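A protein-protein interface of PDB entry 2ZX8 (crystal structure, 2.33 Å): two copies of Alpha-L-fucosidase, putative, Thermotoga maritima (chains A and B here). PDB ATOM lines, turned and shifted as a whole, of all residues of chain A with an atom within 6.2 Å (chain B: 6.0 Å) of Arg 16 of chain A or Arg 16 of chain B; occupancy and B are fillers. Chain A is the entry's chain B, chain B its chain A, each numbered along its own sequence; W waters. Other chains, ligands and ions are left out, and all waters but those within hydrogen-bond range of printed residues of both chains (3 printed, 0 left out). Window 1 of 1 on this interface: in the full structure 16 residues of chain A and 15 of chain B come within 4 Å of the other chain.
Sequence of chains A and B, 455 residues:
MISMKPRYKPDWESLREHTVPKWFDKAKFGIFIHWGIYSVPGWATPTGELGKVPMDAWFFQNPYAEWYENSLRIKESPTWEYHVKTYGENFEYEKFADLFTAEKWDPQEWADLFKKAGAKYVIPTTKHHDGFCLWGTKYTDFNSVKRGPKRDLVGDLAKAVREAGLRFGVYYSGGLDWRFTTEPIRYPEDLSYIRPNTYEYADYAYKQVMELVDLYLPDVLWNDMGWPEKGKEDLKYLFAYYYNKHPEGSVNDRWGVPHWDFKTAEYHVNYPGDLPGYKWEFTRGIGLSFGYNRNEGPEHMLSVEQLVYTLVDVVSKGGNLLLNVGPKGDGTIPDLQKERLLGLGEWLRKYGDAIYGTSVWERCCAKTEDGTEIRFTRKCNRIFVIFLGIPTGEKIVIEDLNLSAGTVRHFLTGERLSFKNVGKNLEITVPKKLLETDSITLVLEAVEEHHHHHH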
ATOM      1  N   TYR A   8     -19.051  21.987  -2.069  1.00  0.00           N
ATOM      2  CA  TYR A   8     -19.846  21.348  -1.034  1.00  0.00           C
ATOM      3  C   TYR A   8     -20.841  22.413  -0.618  1.00  0.00           C
ATOM      4  O   TYR A   8     -20.500  23.611  -0.607  1.00  0.00           O
ATOM      5  CB  TYR A   8     -18.979  20.935   0.159  1.00  0.00           C
ATOM      6  CG  TYR A   8     -17.975  19.865  -0.216  1.00  0.00           C
ATOM      7  CD1 TYR A   8     -18.365  18.516  -0.287  1.00  0.00           C
ATOM      8  CD2 TYR A   8     -16.650  20.201  -0.538  1.00  0.00           C
ATOM      9  CE1 TYR A   8     -17.455  17.517  -0.664  1.00  0.00           C
ATOM     10  CE2 TYR A   8     -15.727  19.230  -0.919  1.00  0.00           C
ATOM     11  CZ  TYR A   8     -16.135  17.883  -0.980  1.00  0.00           C
ATOM     12  OH  TYR A   8     -15.239  16.896  -1.337  1.00  0.00           O
ATOM     13  N   ASP A  11     -24.811  21.798   4.015  1.00  0.00           N
ATOM     14  CA  ASP A  11     -25.808  20.967   4.666  1.00  0.00           C
ATOM     15  C   ASP A  11     -25.223  19.586   4.899  1.00  0.00           C
ATOM     16  O   ASP A  11     -24.333  19.145   4.157  1.00  0.00           O
ATOM     17  CB  ASP A  11     -27.165  20.973   3.959  1.00  0.00           C
ATOM     18  CG  ASP A  11     -27.143  20.305   2.639  1.00  0.00           C
ATOM     19  OD1 ASP A  11     -26.983  21.030   1.631  1.00  0.00           O
ATOM     20  OD2 ASP A  11     -27.326  19.050   2.599  1.00  0.00           O
ATOM     21  N   TRP A  12     -25.625  18.948   6.000  1.00  0.00           N
ATOM     22  CA  TRP A  12     -25.050  17.651   6.343  1.00  0.00           C
ATOM     23  C   TRP A  12     -25.118  16.604   5.230  1.00  0.00           C
ATOM     24  O   TRP A  12     -24.178  15.837   5.063  1.00  0.00           O
ATOM     25  CB  TRP A  12     -25.687  17.081   7.601  1.00  0.00           C
ATOM     26  CG  TRP A  12     -25.702  18.025   8.792  1.00  0.00           C
ATOM     27  CD1 TRP A  12     -26.801  18.437   9.465  1.00  0.00           C
ATOM     28  CD2 TRP A  12     -24.575  18.720   9.393  1.00  0.00           C
ATOM     29  NE1 TRP A  12     -26.450  19.330  10.420  1.00  0.00           N
ATOM     30  CE2 TRP A  12     -25.105  19.542  10.409  1.00  0.00           C
ATOM     31  CE3 TRP A  12     -23.186  18.727   9.158  1.00  0.00           C
ATOM     32  CZ2 TRP A  12     -24.323  20.383  11.198  1.00  0.00           C
ATOM     33  CZ3 TRP A  12     -22.377  19.575   9.946  1.00  0.00           C
ATOM     34  CH2 TRP A  12     -22.958  20.397  10.952  1.00  0.00           C
ATOM     35  N   GLU A  13     -26.187  16.613   4.448  1.00  0.00           N
ATOM     36  CA  GLU A  13     -26.392  15.633   3.370  1.00  0.00           C
ATOM     37  C   GLU A  13     -25.370  15.843   2.265  1.00  0.00           C
ATOM     38  O   GLU A  13     -24.904  14.901   1.645  1.00  0.00           O
ATOM     39  CB  GLU A  13     -27.841  15.726   2.813  1.00  0.00           C
ATOM     40  CG  GLU A  13     -28.209  14.609   1.872  1.00  0.00           C
ATOM     41  CD  GLU A  13     -29.725  14.517   1.387  1.00  0.00           C
ATOM     42  OE1 GLU A  13     -30.055  13.486   0.742  1.00  0.00           O
ATOM     43  OE2 GLU A  13     -30.574  15.433   1.628  1.00  0.00           O
ATOM     44  N   SER A  14     -24.999  17.087   2.043  1.00  0.00           N
ATOM     45  CA  SER A  14     -24.028  17.403   1.020  1.00  0.00           C
ATOM     46  C   SER A  14     -22.615  17.173   1.543  1.00  0.00           C
ATOM     47  O   SER A  14     -21.795  16.538   0.865  1.00  0.00           O
ATOM     48  CB  SER A  14     -24.214  18.855   0.581  1.00  0.00           C
ATOM     49  OG  SER A  14     -23.076  19.303  -0.122  1.00  0.00           O
ATOM     50  N   LEU A  15     -22.339  17.654   2.769  1.00  0.00           N
ATOM     51  CA  LEU A  15     -21.019  17.480   3.361  1.00  0.00           C
ATOM     52  C   LEU A  15     -20.621  16.005   3.501  1.00  0.00           C
ATOM     53  O   LEU A  15     -19.431  15.704   3.521  1.00  0.00           O
ATOM     54  CB  LEU A  15     -20.968  18.153   4.712  1.00  0.00           C
ATOM     55  CG  LEU A  15     -21.012  19.696   4.707  1.00  0.00           C
ATOM     56  CD1 LEU A  15     -21.389  20.210   6.144  1.00  0.00           C
ATOM     57  CD2 LEU A  15     -19.647  20.240   4.214  1.00  0.00           C
ATOM     58  N   ARG A  16     -21.606  15.091   3.578  1.00  0.00           N
ATOM     59  CA  ARG A  16     -21.342  13.637   3.665  1.00  0.00           C
ATOM     60  C   ARG A  16     -20.564  13.136   2.432  1.00  0.00           C
ATOM     61  O   ARG A  16     -19.916  12.111   2.489  1.00  0.00           O
ATOM     62  CB  ARG A  16     -22.650  12.822   3.792  1.00  0.00           C
ATOM     63  CG  ARG A  16     -22.552  11.404   3.094  1.00  0.00           C
ATOM     64  CD  ARG A  16     -23.299  10.216   3.741  1.00  0.00           C
ATOM     65  NE  ARG A  16     -22.494   9.692   4.839  1.00  0.00           N
ATOM     66  CZ  ARG A  16     -22.175   8.418   5.059  1.00  0.00           C
ATOM     67  NH1 ARG A  16     -22.590   7.415   4.255  1.00  0.00           N
ATOM     68  NH2 ARG A  16     -21.405   8.174   6.101  1.00  0.00           N
ATOM     69  N   GLU A  17     -20.701  13.847   1.316  1.00  0.00           N
ATOM     70  CA  GLU A  17     -19.974  13.545   0.087  1.00  0.00           C
ATOM     71  C   GLU A  17     -18.466  13.569   0.313  1.00  0.00           C
ATOM     72  O   GLU A  17     -17.713  12.997  -0.480  1.00  0.00           O
ATOM     73  CB  GLU A  17     -20.284  14.586  -1.006  1.00  0.00           C
ATOM     74  CG  GLU A  17     -21.629  14.383  -1.623  1.00  0.00           C
ATOM     75  CD  GLU A  17     -22.073  15.456  -2.591  1.00  0.00           C
ATOM     76  OE1 GLU A  17     -23.287  15.547  -2.827  1.00  0.00           O
ATOM     77  OE2 GLU A  17     -21.251  16.210  -3.130  1.00  0.00           O
ATOM     78  N   HIS A  18     -18.013  14.248   1.367  1.00  0.00           N
ATOM     79  CA  HIS A  18     -16.585  14.315   1.603  1.00  0.00           C
ATOM     80  C   HIS A  18     -16.173  13.199   2.557  1.00  0.00           C
ATOM     81  O   HIS A  18     -16.706  13.063   3.654  1.00  0.00           O
ATOM     82  CB  HIS A  18     -16.235  15.726   2.122  1.00  0.00           C
ATOM     83  CG  HIS A  18     -14.852  15.854   2.641  1.00  0.00           C
ATOM     84  ND1 HIS A  18     -14.460  15.297   3.839  1.00  0.00           N
ATOM     85  CD2 HIS A  18     -13.731  16.363   2.073  1.00  0.00           C
ATOM     86  CE1 HIS A  18     -13.152  15.442   3.978  1.00  0.00           C
ATOM     87  NE2 HIS A  18     -12.684  16.081   2.918  1.00  0.00           N
ATOM     88  N   THR A  19     -15.243  12.370   2.130  1.00  0.00           N
ATOM     89  CA  THR A  19     -14.794  11.293   2.961  1.00  0.00           C
ATOM     90  C   THR A  19     -13.352  11.504   3.343  1.00  0.00           C
ATOM     91  O   THR A  19     -12.717  12.408   2.839  1.00  0.00           O
ATOM     92  CB  THR A  19     -14.990   9.942   2.264  1.00  0.00           C
ATOM     93  OG1 THR A  19     -14.575  10.041   0.884  1.00  0.00           O
ATOM     94  CG2 THR A  19     -16.470   9.560   2.299  1.00  0.00           C
ATOM     95  N   VAL A  20     -12.844  10.689   4.265  1.00  0.00           N
ATOM     96  CA  VAL A  20     -11.493  10.865   4.698  1.00  0.00           C
ATOM     97  C   VAL A  20     -10.601  10.842   3.466  1.00  0.00           C
ATOM     98  O   VAL A  20     -10.784  10.022   2.593  1.00  0.00           O
ATOM     99  CB  VAL A  20     -11.123   9.763   5.708  1.00  0.00           C
ATOM    100  CG1 VAL A  20     -11.228   8.384   5.065  1.00  0.00           C
ATOM    101  CG2 VAL A  20      -9.764  10.049   6.295  1.00  0.00           C
ATOM    102  N   PRO A 258     -23.552  15.831  12.925  1.00  0.00           N
ATOM    103  CA  PRO A 258     -23.594  14.659  12.028  1.00  0.00           C
ATOM    104  C   PRO A 258     -22.330  14.302  11.228  1.00  0.00           C
ATOM    105  O   PRO A 258     -22.044  13.133  10.973  1.00  0.00           O
ATOM    106  CB  PRO A 258     -24.760  14.983  11.091  1.00  0.00           C
ATOM    107  CG  PRO A 258     -25.674  15.748  11.964  1.00  0.00           C
ATOM    108  CD  PRO A 258     -24.711  16.706  12.685  1.00  0.00           C
ATOM    109  N   HIS A 259     -21.543  15.285  10.867  1.00  0.00           N
ATOM    110  CA  HIS A 259     -20.368  15.038  10.056  1.00  0.00           C
ATOM    111  C   HIS A 259     -19.013  14.823  10.715  1.00  0.00           C
ATOM    112  O   HIS A 259     -18.711  15.386  11.754  1.00  0.00           O
ATOM    113  CB  HIS A 259     -20.257  16.170   9.045  1.00  0.00           C
ATOM    114  CG  HIS A 259     -19.262  15.892   7.973  1.00  0.00           C
ATOM    115  ND1 HIS A 259     -19.463  14.908   7.028  1.00  0.00           N
ATOM    116  CD2 HIS A 259     -18.009  16.368   7.777  1.00  0.00           C
ATOM    117  CE1 HIS A 259     -18.373  14.783   6.299  1.00  0.00           C
ATOM    118  NE2 HIS A 259     -17.472  15.654   6.729  1.00  0.00           N
ATOM    119  N   TRP A 260     -18.193  13.974  10.109  1.00  0.00           N
ATOM    120  CA  TRP A 260     -16.822  13.736  10.597  1.00  0.00           C
ATOM    121  C   TRP A 260     -16.125  12.902   9.523  1.00  0.00           C
ATOM    122  O   TRP A 260     -16.776  12.184   8.809  1.00  0.00           O
ATOM    123  CB  TRP A 260     -16.784  13.010  11.965  1.00  0.00           C
ATOM    124  CG  TRP A 260     -17.653  11.759  12.077  1.00  0.00           C
ATOM    125  CD1 TRP A 260     -18.940  11.687  12.578  1.00  0.00           C
ATOM    126  CD2 TRP A 260     -17.334  10.425  11.614  1.00  0.00           C
ATOM    127  NE1 TRP A 260     -19.434  10.402  12.448  1.00  0.00           N
ATOM    128  CE2 TRP A 260     -18.480   9.609  11.859  1.00  0.00           C
ATOM    129  CE3 TRP A 260     -16.206   9.840  11.022  1.00  0.00           C
ATOM    130  CZ2 TRP A 260     -18.519   8.247  11.526  1.00  0.00           C
ATOM    131  CZ3 TRP A 260     -16.250   8.461  10.680  1.00  0.00           C
ATOM    132  CH2 TRP A 260     -17.404   7.688  10.938  1.00  0.00           C
ATOM    133  N   ASP A 261     -14.806  12.993   9.408  1.00  0.00           N
ATOM    134  CA  ASP A 261     -14.107  12.194   8.409  1.00  0.00           C
ATOM    135  C   ASP A 261     -13.476  10.969   9.065  1.00  0.00           C
ATOM    136  O   ASP A 261     -13.270   9.954   8.408  1.00  0.00           O
ATOM    137  CB  ASP A 261     -13.028  13.037   7.708  1.00  0.00           C
ATOM    138  CG  ASP A 261     -13.636  14.140   6.853  1.00  0.00           C
ATOM    139  OD1 ASP A 261     -13.181  15.318   6.955  1.00  0.00           O
ATOM    140  OD2 ASP A 261     -14.569  13.814   6.073  1.00  0.00           O
ATOM    141  N   TYR A 278     -15.007   1.815  10.081  1.00  0.00           N
ATOM    142  CA  TYR A 278     -14.836   3.219   9.639  1.00  0.00           C
ATOM    143  C   TYR A 278     -13.438   3.658   9.976  1.00  0.00           C
ATOM    144  O   TYR A 278     -12.809   3.060  10.829  1.00  0.00           O
ATOM    145  CB  TYR A 278     -15.822   4.130  10.376  1.00  0.00           C
ATOM    146  CG  TYR A 278     -15.856   3.895  11.884  1.00  0.00           C
ATOM    147  CD1 TYR A 278     -14.900   4.449  12.718  1.00  0.00           C
ATOM    148  CD2 TYR A 278     -16.842   3.084  12.456  1.00  0.00           C
ATOM    149  CE1 TYR A 278     -14.925   4.202  14.102  1.00  0.00           C
ATOM    150  CE2 TYR A 278     -16.880   2.836  13.783  1.00  0.00           C
ATOM    151  CZ  TYR A 278     -15.938   3.381  14.610  1.00  0.00           C
ATOM    152  OH  TYR A 278     -15.986   3.082  15.927  1.00  0.00           O
ATOM    153  N   ASP B  11     -28.955   7.906  15.416  1.00  0.00           N
ATOM    154  CA  ASP B  11     -28.636   9.323  15.212  1.00  0.00           C
ATOM    155  C   ASP B  11     -27.664   9.391  14.012  1.00  0.00           C
ATOM    156  O   ASP B  11     -26.915   8.443  13.719  1.00  0.00           O
ATOM    157  CB  ASP B  11     -28.065  10.002  16.449  1.00  0.00           C
ATOM    158  CG  ASP B  11     -26.718   9.571  16.714  1.00  0.00           C
ATOM    159  OD1 ASP B  11     -26.649   8.668  17.540  1.00  0.00           O
ATOM    160  OD2 ASP B  11     -25.736  10.090  16.087  1.00  0.00           O
ATOM    161  N   TRP B  12     -27.739  10.506  13.309  1.00  0.00           N
ATOM    162  CA  TRP B  12     -26.969  10.683  12.088  1.00  0.00           C
ATOM    163  C   TRP B  12     -25.484  10.511  12.232  1.00  0.00           C
ATOM    164  O   TRP B  12     -24.845   9.998  11.325  1.00  0.00           O
ATOM    165  CB  TRP B  12     -27.262  12.048  11.495  1.00  0.00           C
ATOM    166  CG  TRP B  12     -28.691  12.306  11.374  1.00  0.00           C
ATOM    167  CD1 TRP B  12     -29.370  13.312  11.945  1.00  0.00           C
ATOM    168  CD2 TRP B  12     -29.646  11.540  10.617  1.00  0.00           C
ATOM    169  NE1 TRP B  12     -30.687  13.247  11.599  1.00  0.00           N
ATOM    170  CE2 TRP B  12     -30.895  12.168  10.785  1.00  0.00           C
ATOM    171  CE3 TRP B  12     -29.566  10.386   9.823  1.00  0.00           C
ATOM    172  CZ2 TRP B  12     -32.079  11.690  10.186  1.00  0.00           C
ATOM    173  CZ3 TRP B  12     -30.729   9.908   9.229  1.00  0.00           C
ATOM    174  CH2 TRP B  12     -31.981  10.566   9.418  1.00  0.00           C
ATOM    175  N   GLU B  13     -24.952  10.883  13.396  1.00  0.00           N
ATOM    176  CA  GLU B  13     -23.513  10.799  13.640  1.00  0.00           C
ATOM    177  C   GLU B  13     -23.033   9.341  13.726  1.00  0.00           C
ATOM    178  O   GLU B  13     -21.926   9.004  13.297  1.00  0.00           O
ATOM    179  CB  GLU B  13     -23.146  11.595  14.922  1.00  0.00           C
ATOM    180  CG  GLU B  13     -21.688  11.772  15.127  1.00  0.00           C
ATOM    181  CD  GLU B  13     -21.256  12.828  16.203  1.00  0.00           C
ATOM    182  OE1 GLU B  13     -20.044  13.226  16.144  1.00  0.00           O
ATOM    183  OE2 GLU B  13     -22.081  13.237  17.091  1.00  0.00           O
ATOM    184  N   SER B  14     -23.867   8.491  14.305  1.00  0.00           N
ATOM    185  CA  SER B  14     -23.546   7.064  14.445  1.00  0.00           C
ATOM    186  C   SER B  14     -23.776   6.337  13.108  1.00  0.00           C
ATOM    187  O   SER B  14     -22.946   5.509  12.658  1.00  0.00           O
ATOM    188  CB  SER B  14     -24.434   6.417  15.529  1.00  0.00           C
ATOM    189  OG  SER B  14     -24.395   5.000  15.378  1.00  0.00           O
ATOM    190  N   LEU B  15     -24.896   6.686  12.465  1.00  0.00           N
ATOM    191  CA  LEU B  15     -25.241   6.072  11.188  1.00  0.00           C
ATOM    192  C   LEU B  15     -24.165   6.363  10.118  1.00  0.00           C
ATOM    193  O   LEU B  15     -23.937   5.557   9.225  1.00  0.00           O
ATOM    194  CB  LEU B  15     -26.642   6.527  10.742  1.00  0.00           C
ATOM    195  CG  LEU B  15     -27.732   5.938  11.673  1.00  0.00           C
ATOM    196  CD1 LEU B  15     -29.063   6.673  11.385  1.00  0.00           C
ATOM    197  CD2 LEU B  15     -27.874   4.359  11.497  1.00  0.00           C
ATOM    198  N   ARG B  16     -23.496   7.499  10.255  1.00  0.00           N
ATOM    199  CA  ARG B  16     -22.412   7.931   9.340  1.00  0.00           C
ATOM    200  C   ARG B  16     -21.317   6.830   9.233  1.00  0.00           C
ATOM    201  O   ARG B  16     -20.682   6.653   8.202  1.00  0.00           O
ATOM    202  CB  ARG B  16     -21.844   9.231   9.904  1.00  0.00           C
ATOM    203  CG  ARG B  16     -20.464   9.646   9.464  1.00  0.00           C
ATOM    204  CD  ARG B  16     -20.419  10.180   8.025  1.00  0.00           C
ATOM    205  NE  ARG B  16     -19.069  10.511   7.561  1.00  0.00           N
ATOM    206  CZ  ARG B  16     -18.830  10.948   6.326  1.00  0.00           C
ATOM    207  NH1 ARG B  16     -19.870  11.052   5.496  1.00  0.00           N
ATOM    208  NH2 ARG B  16     -17.584  11.340   5.944  1.00  0.00           N
ATOM    209  N   GLU B  17     -21.128   6.093  10.319  1.00  0.00           N
ATOM    210  CA  GLU B  17     -20.204   4.982  10.382  1.00  0.00           C
ATOM    211  C   GLU B  17     -20.473   3.904   9.340  1.00  0.00           C
ATOM    212  O   GLU B  17     -19.589   3.132   9.055  1.00  0.00           O
ATOM    213  CB  GLU B  17     -20.279   4.301  11.750  1.00  0.00           C
ATOM    214  CG  GLU B  17     -19.796   5.161  12.897  1.00  0.00           C
ATOM    215  CD  GLU B  17     -19.950   4.448  14.202  1.00  0.00           C
ATOM    216  OE1 GLU B  17     -19.878   5.086  15.274  1.00  0.00           O
ATOM    217  OE2 GLU B  17     -20.156   3.204  14.136  1.00  0.00           O
ATOM    218  N   HIS B  18     -21.707   3.803   8.841  1.00  0.00           N
ATOM    219  CA  HIS B  18     -22.023   2.801   7.871  1.00  0.00           C
ATOM    220  C   HIS B  18     -21.755   3.349   6.535  1.00  0.00           C
ATOM    221  O   HIS B  18     -22.270   4.394   6.179  1.00  0.00           O
ATOM    222  CB  HIS B  18     -23.507   2.389   7.941  1.00  0.00           C
ATOM    223  CG  HIS B  18     -23.891   1.354   6.917  1.00  0.00           C
ATOM    224  ND1 HIS B  18     -24.235   1.674   5.609  1.00  0.00           N
ATOM    225  CD2 HIS B  18     -23.939  -0.004   7.004  1.00  0.00           C
ATOM    226  CE1 HIS B  18     -24.482   0.562   4.942  1.00  0.00           C
ATOM    227  NE2 HIS B  18     -24.313  -0.469   5.767  1.00  0.00           N
ATOM    228  N   THR B  19     -20.930   2.676   5.777  1.00  0.00           N
ATOM    229  CA  THR B  19     -20.690   3.128   4.421  1.00  0.00           C
ATOM    230  C   THR B  19     -21.091   2.040   3.446  1.00  0.00           C
ATOM    231  O   THR B  19     -21.406   0.909   3.848  1.00  0.00           O
ATOM    232  CB  THR B  19     -19.209   3.533   4.165  1.00  0.00           C
ATOM    233  OG1 THR B  19     -18.354   2.483   4.587  1.00  0.00           O
ATOM    234  CG2 THR B  19     -18.882   4.846   4.933  1.00  0.00           C
ATOM    235  N   VAL B  20     -21.060   2.390   2.167  1.00  0.00           N
ATOM    236  CA  VAL B  20     -21.442   1.469   1.121  1.00  0.00           C
ATOM    237  C   VAL B  20     -20.733   0.148   1.277  1.00  0.00           C
ATOM    238  O   VAL B  20     -19.515   0.076   1.415  1.00  0.00           O
ATOM    239  CB  VAL B  20     -21.177   2.037  -0.317  1.00  0.00           C
ATOM    240  CG1 VAL B  20     -19.643   2.007  -0.662  1.00  0.00           C
ATOM    241  CG2 VAL B  20     -21.984   1.234  -1.350  1.00  0.00           C
ATOM    242  N   PRO B 258     -29.687  13.545   6.348  1.00  0.00           N
ATOM    243  CA  PRO B 258     -28.223  13.516   6.266  1.00  0.00           C
ATOM    244  C   PRO B 258     -27.599  12.235   5.742  1.00  0.00           C
ATOM    245  O   PRO B 258     -26.721  12.305   4.942  1.00  0.00           O
ATOM    246  CB  PRO B 258     -27.772  13.852   7.696  1.00  0.00           C
ATOM    247  CG  PRO B 258     -28.840  14.854   8.139  1.00  0.00           C
ATOM    248  CD  PRO B 258     -30.110  14.110   7.645  1.00  0.00           C
ATOM    249  N   HIS B 259     -28.097  11.075   6.096  1.00  0.00           N
ATOM    250  CA  HIS B 259     -27.469   9.832   5.647  1.00  0.00           C
ATOM    251  C   HIS B 259     -27.891   9.272   4.281  1.00  0.00           C
ATOM    252  O   HIS B 259     -29.013   9.511   3.815  1.00  0.00           O
ATOM    253  CB  HIS B 259     -27.704   8.755   6.734  1.00  0.00           C
ATOM    254  CG  HIS B 259     -26.883   7.513   6.546  1.00  0.00           C
ATOM    255  ND1 HIS B 259     -25.513   7.493   6.723  1.00  0.00           N
ATOM    256  CD2 HIS B 259     -27.225   6.275   6.091  1.00  0.00           C
ATOM    257  CE1 HIS B 259     -25.040   6.305   6.379  1.00  0.00           C
ATOM    258  NE2 HIS B 259     -26.054   5.544   5.988  1.00  0.00           N
ATOM    259  N   TRP B 260     -26.960   8.529   3.672  1.00  0.00           N
ATOM    260  CA  TRP B 260     -27.122   7.807   2.412  1.00  0.00           C
ATOM    261  C   TRP B 260     -25.796   7.034   2.230  1.00  0.00           C
ATOM    262  O   TRP B 260     -24.775   7.464   2.759  1.00  0.00           O
ATOM    263  CB  TRP B 260     -27.390   8.747   1.208  1.00  0.00           C
ATOM    264  CG  TRP B 260     -26.423   9.881   1.079  1.00  0.00           C
ATOM    265  CD1 TRP B 260     -26.606  11.180   1.510  1.00  0.00           C
ATOM    266  CD2 TRP B 260     -25.126   9.849   0.476  1.00  0.00           C
ATOM    267  NE1 TRP B 260     -25.513  11.949   1.202  1.00  0.00           N
ATOM    268  CE2 TRP B 260     -24.582  11.168   0.581  1.00  0.00           C
ATOM    269  CE3 TRP B 260     -24.369   8.847  -0.142  1.00  0.00           C
ATOM    270  CZ2 TRP B 260     -23.313  11.511   0.098  1.00  0.00           C
ATOM    271  CZ3 TRP B 260     -23.074   9.191  -0.637  1.00  0.00           C
ATOM    272  CH2 TRP B 260     -22.563  10.514  -0.510  1.00  0.00           C
ATOM    273  N   ASP B 261     -25.828   5.898   1.526  1.00  0.00           N
ATOM    274  CA  ASP B 261     -24.643   5.096   1.268  1.00  0.00           C
ATOM    275  C   ASP B 261     -24.133   5.338  -0.177  1.00  0.00           C
ATOM    276  O   ASP B 261     -22.959   5.119  -0.445  1.00  0.00           O
ATOM    277  CB  ASP B 261     -24.913   3.596   1.438  1.00  0.00           C
ATOM    278  CG  ASP B 261     -25.222   3.229   2.842  1.00  0.00           C
ATOM    279  OD1 ASP B 261     -26.229   2.491   2.998  1.00  0.00           O
ATOM    280  OD2 ASP B 261     -24.467   3.648   3.785  1.00  0.00           O
ATOM    281  N   TYR B 278     -17.472  10.015  -4.586  1.00  0.00           N
ATOM    282  CA  TYR B 278     -18.295   9.163  -3.716  1.00  0.00           C
ATOM    283  C   TYR B 278     -18.972   8.138  -4.584  1.00  0.00           C
ATOM    284  O   TYR B 278     -19.080   8.353  -5.771  1.00  0.00           O
ATOM    285  CB  TYR B 278     -19.373  10.008  -3.036  1.00  0.00           C
ATOM    286  CG  TYR B 278     -20.013  10.993  -3.981  1.00  0.00           C
ATOM    287  CD1 TYR B 278     -20.991  10.599  -4.874  1.00  0.00           C
ATOM    288  CD2 TYR B 278     -19.608  12.339  -4.007  1.00  0.00           C
ATOM    289  CE1 TYR B 278     -21.565  11.513  -5.769  1.00  0.00           C
ATOM    290  CE2 TYR B 278     -20.175  13.254  -4.908  1.00  0.00           C
ATOM    291  CZ  TYR B 278     -21.141  12.826  -5.757  1.00  0.00           C
ATOM    292  OH  TYR B 278     -21.765  13.726  -6.560  1.00  0.00           O
HETATM  293  O   HOH W   1     -18.520  15.246  15.152  1.00  0.00           O
HETATM  294  O   HOH W   2     -15.392   8.862   6.267  1.00  0.00           O
HETATM  295  O   HOH W   3     -31.071  10.785   1.645  1.00  0.00           O
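The guanidinium group of Arg 16 of chain B lies within hydrogen-bond range of the backbone carbonyl oxygen of Trp 260 of chain A (3.1 Å).
NH2 of Arg 16 of chain B lies within hydrogen-bond range of O of His 18 of chain A (3.0 Å).
The side-chain carboxylate (OD2) of Asp 261 of chain A lies within salt-bridge range of the guanidinium group (NH2) of Arg 16 of chain B (3.9 Å).
The guanidinium group (NH2) of Arg 16 of chain A is in hydrogen-bond range of the backbone carbonyl oxygen (O) of Arg 16 of chain B (2.7 Å).
NE1 of Trp 260 of chain A is in hydrogen-bond range of O of Glu 13 of chain B.
The indole nitrogen of Trp 260 of chain B is in hydrogen-bond range of the backbone carbonyl oxygen of Glu 13 of chain A (3.0 Å).
O of Trp 260 of chain B is in hydrogen-bond range of NH1 of Arg 16 of chain A (2.6 Å).
A ring nitrogen (NE2) of His 259 of chain B sits at hydrogen-bond distance from the side-chain carboxylate (OD2) of Asp 261 of chain B (3.3 Å).
A ring nitrogen (ND1) of His 18 of chain B sits at hydrogen-bond distance from the side-chain carboxylate (OD2) of Asp 261 of chain B (2.7 Å).
Among the printed residues, merely in contact across the chains: Tyr 278 of chain A with Glu 17 of chain B (3.3 Å), Arg 16 of chain A with His 259 of chain B (3.4 Å), His 259 of chain A with Arg 16 of chain B (3.6 Å), Trp 260 of chain A with Glu 17 of chain B (3.6 Å), Arg 16 of chain A with His 18 of chain B (3.6 Å), Glu 17 of chain A with Tyr 278 of chain B (3.6 Å), Glu 13 of chain A with Pro 258 of chain B (3.7 Å), Glu 17 of chain A with Trp 260 of chain B (3.7 Å), Pro 258 of chain A with Glu 13 of chain B (3.8 Å), Trp 12 of chain A with Pro 258 of chain B (3.8 Å) and Pro 258 of chain A with Trp 12 of chain B (3.9 Å).
Of the printed residues of chain A, Arg 16 of chain B touches Arg 16 (2.7 Å), His 18 (3.0 Å), His 259 (3.6 Å), Trp 260 (3.1 Å) and Asp 261 (3.9 Å).
Printed residues of chain A within 4 Å of Glu 13 of chain B: Pro 258 (3.8 Å) and Trp 260 (3.0 Å).
Printed residues of chain A within 4 Å of Pro 258 of chain B: Trp 12 and Glu 13.
Of the 16 printed residues of chain A, 10 touch a printed residue of chain B.
Hydrophobic or aromatic side chains of chain B that line the printed part of chain A: Trp 12, Pro 258, His 259, Trp 260 and Tyr 278.
Among the printed residues, Asp or Glu carboxylates within 4 Å of a Lys or Arg side-chain nitrogen of the other chain: Asp 261 of chain A with Arg 16 of chain B.
Trp 12 of chain A touches Pro 258 of chain B, and with the chains exchanged Pro 258 of chain A touches Trp 12 of chain B.
Arg 16 of chain A touches His 18 of chain B, and with the chains exchanged His 18 of chain A touches Arg 16 of chain B.
15 positions are printed for both chains.
Water W1 lies within hydrogen-bond range of OE1 of Glu 13 of chain B and O of His 259 of chain A.
Water W3 bridges the side-chain carboxylate of Glu 13 of chain A (3.0 Å) and the backbone carbonyl oxygen of His 259 of chain B (3.3 Å).
Water W2 bridges the backbone carbonyl oxygen of Asp 261 of chain A (3.2 Å) and the guanidinium group of Arg 16 of chain B (3.3 Å).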
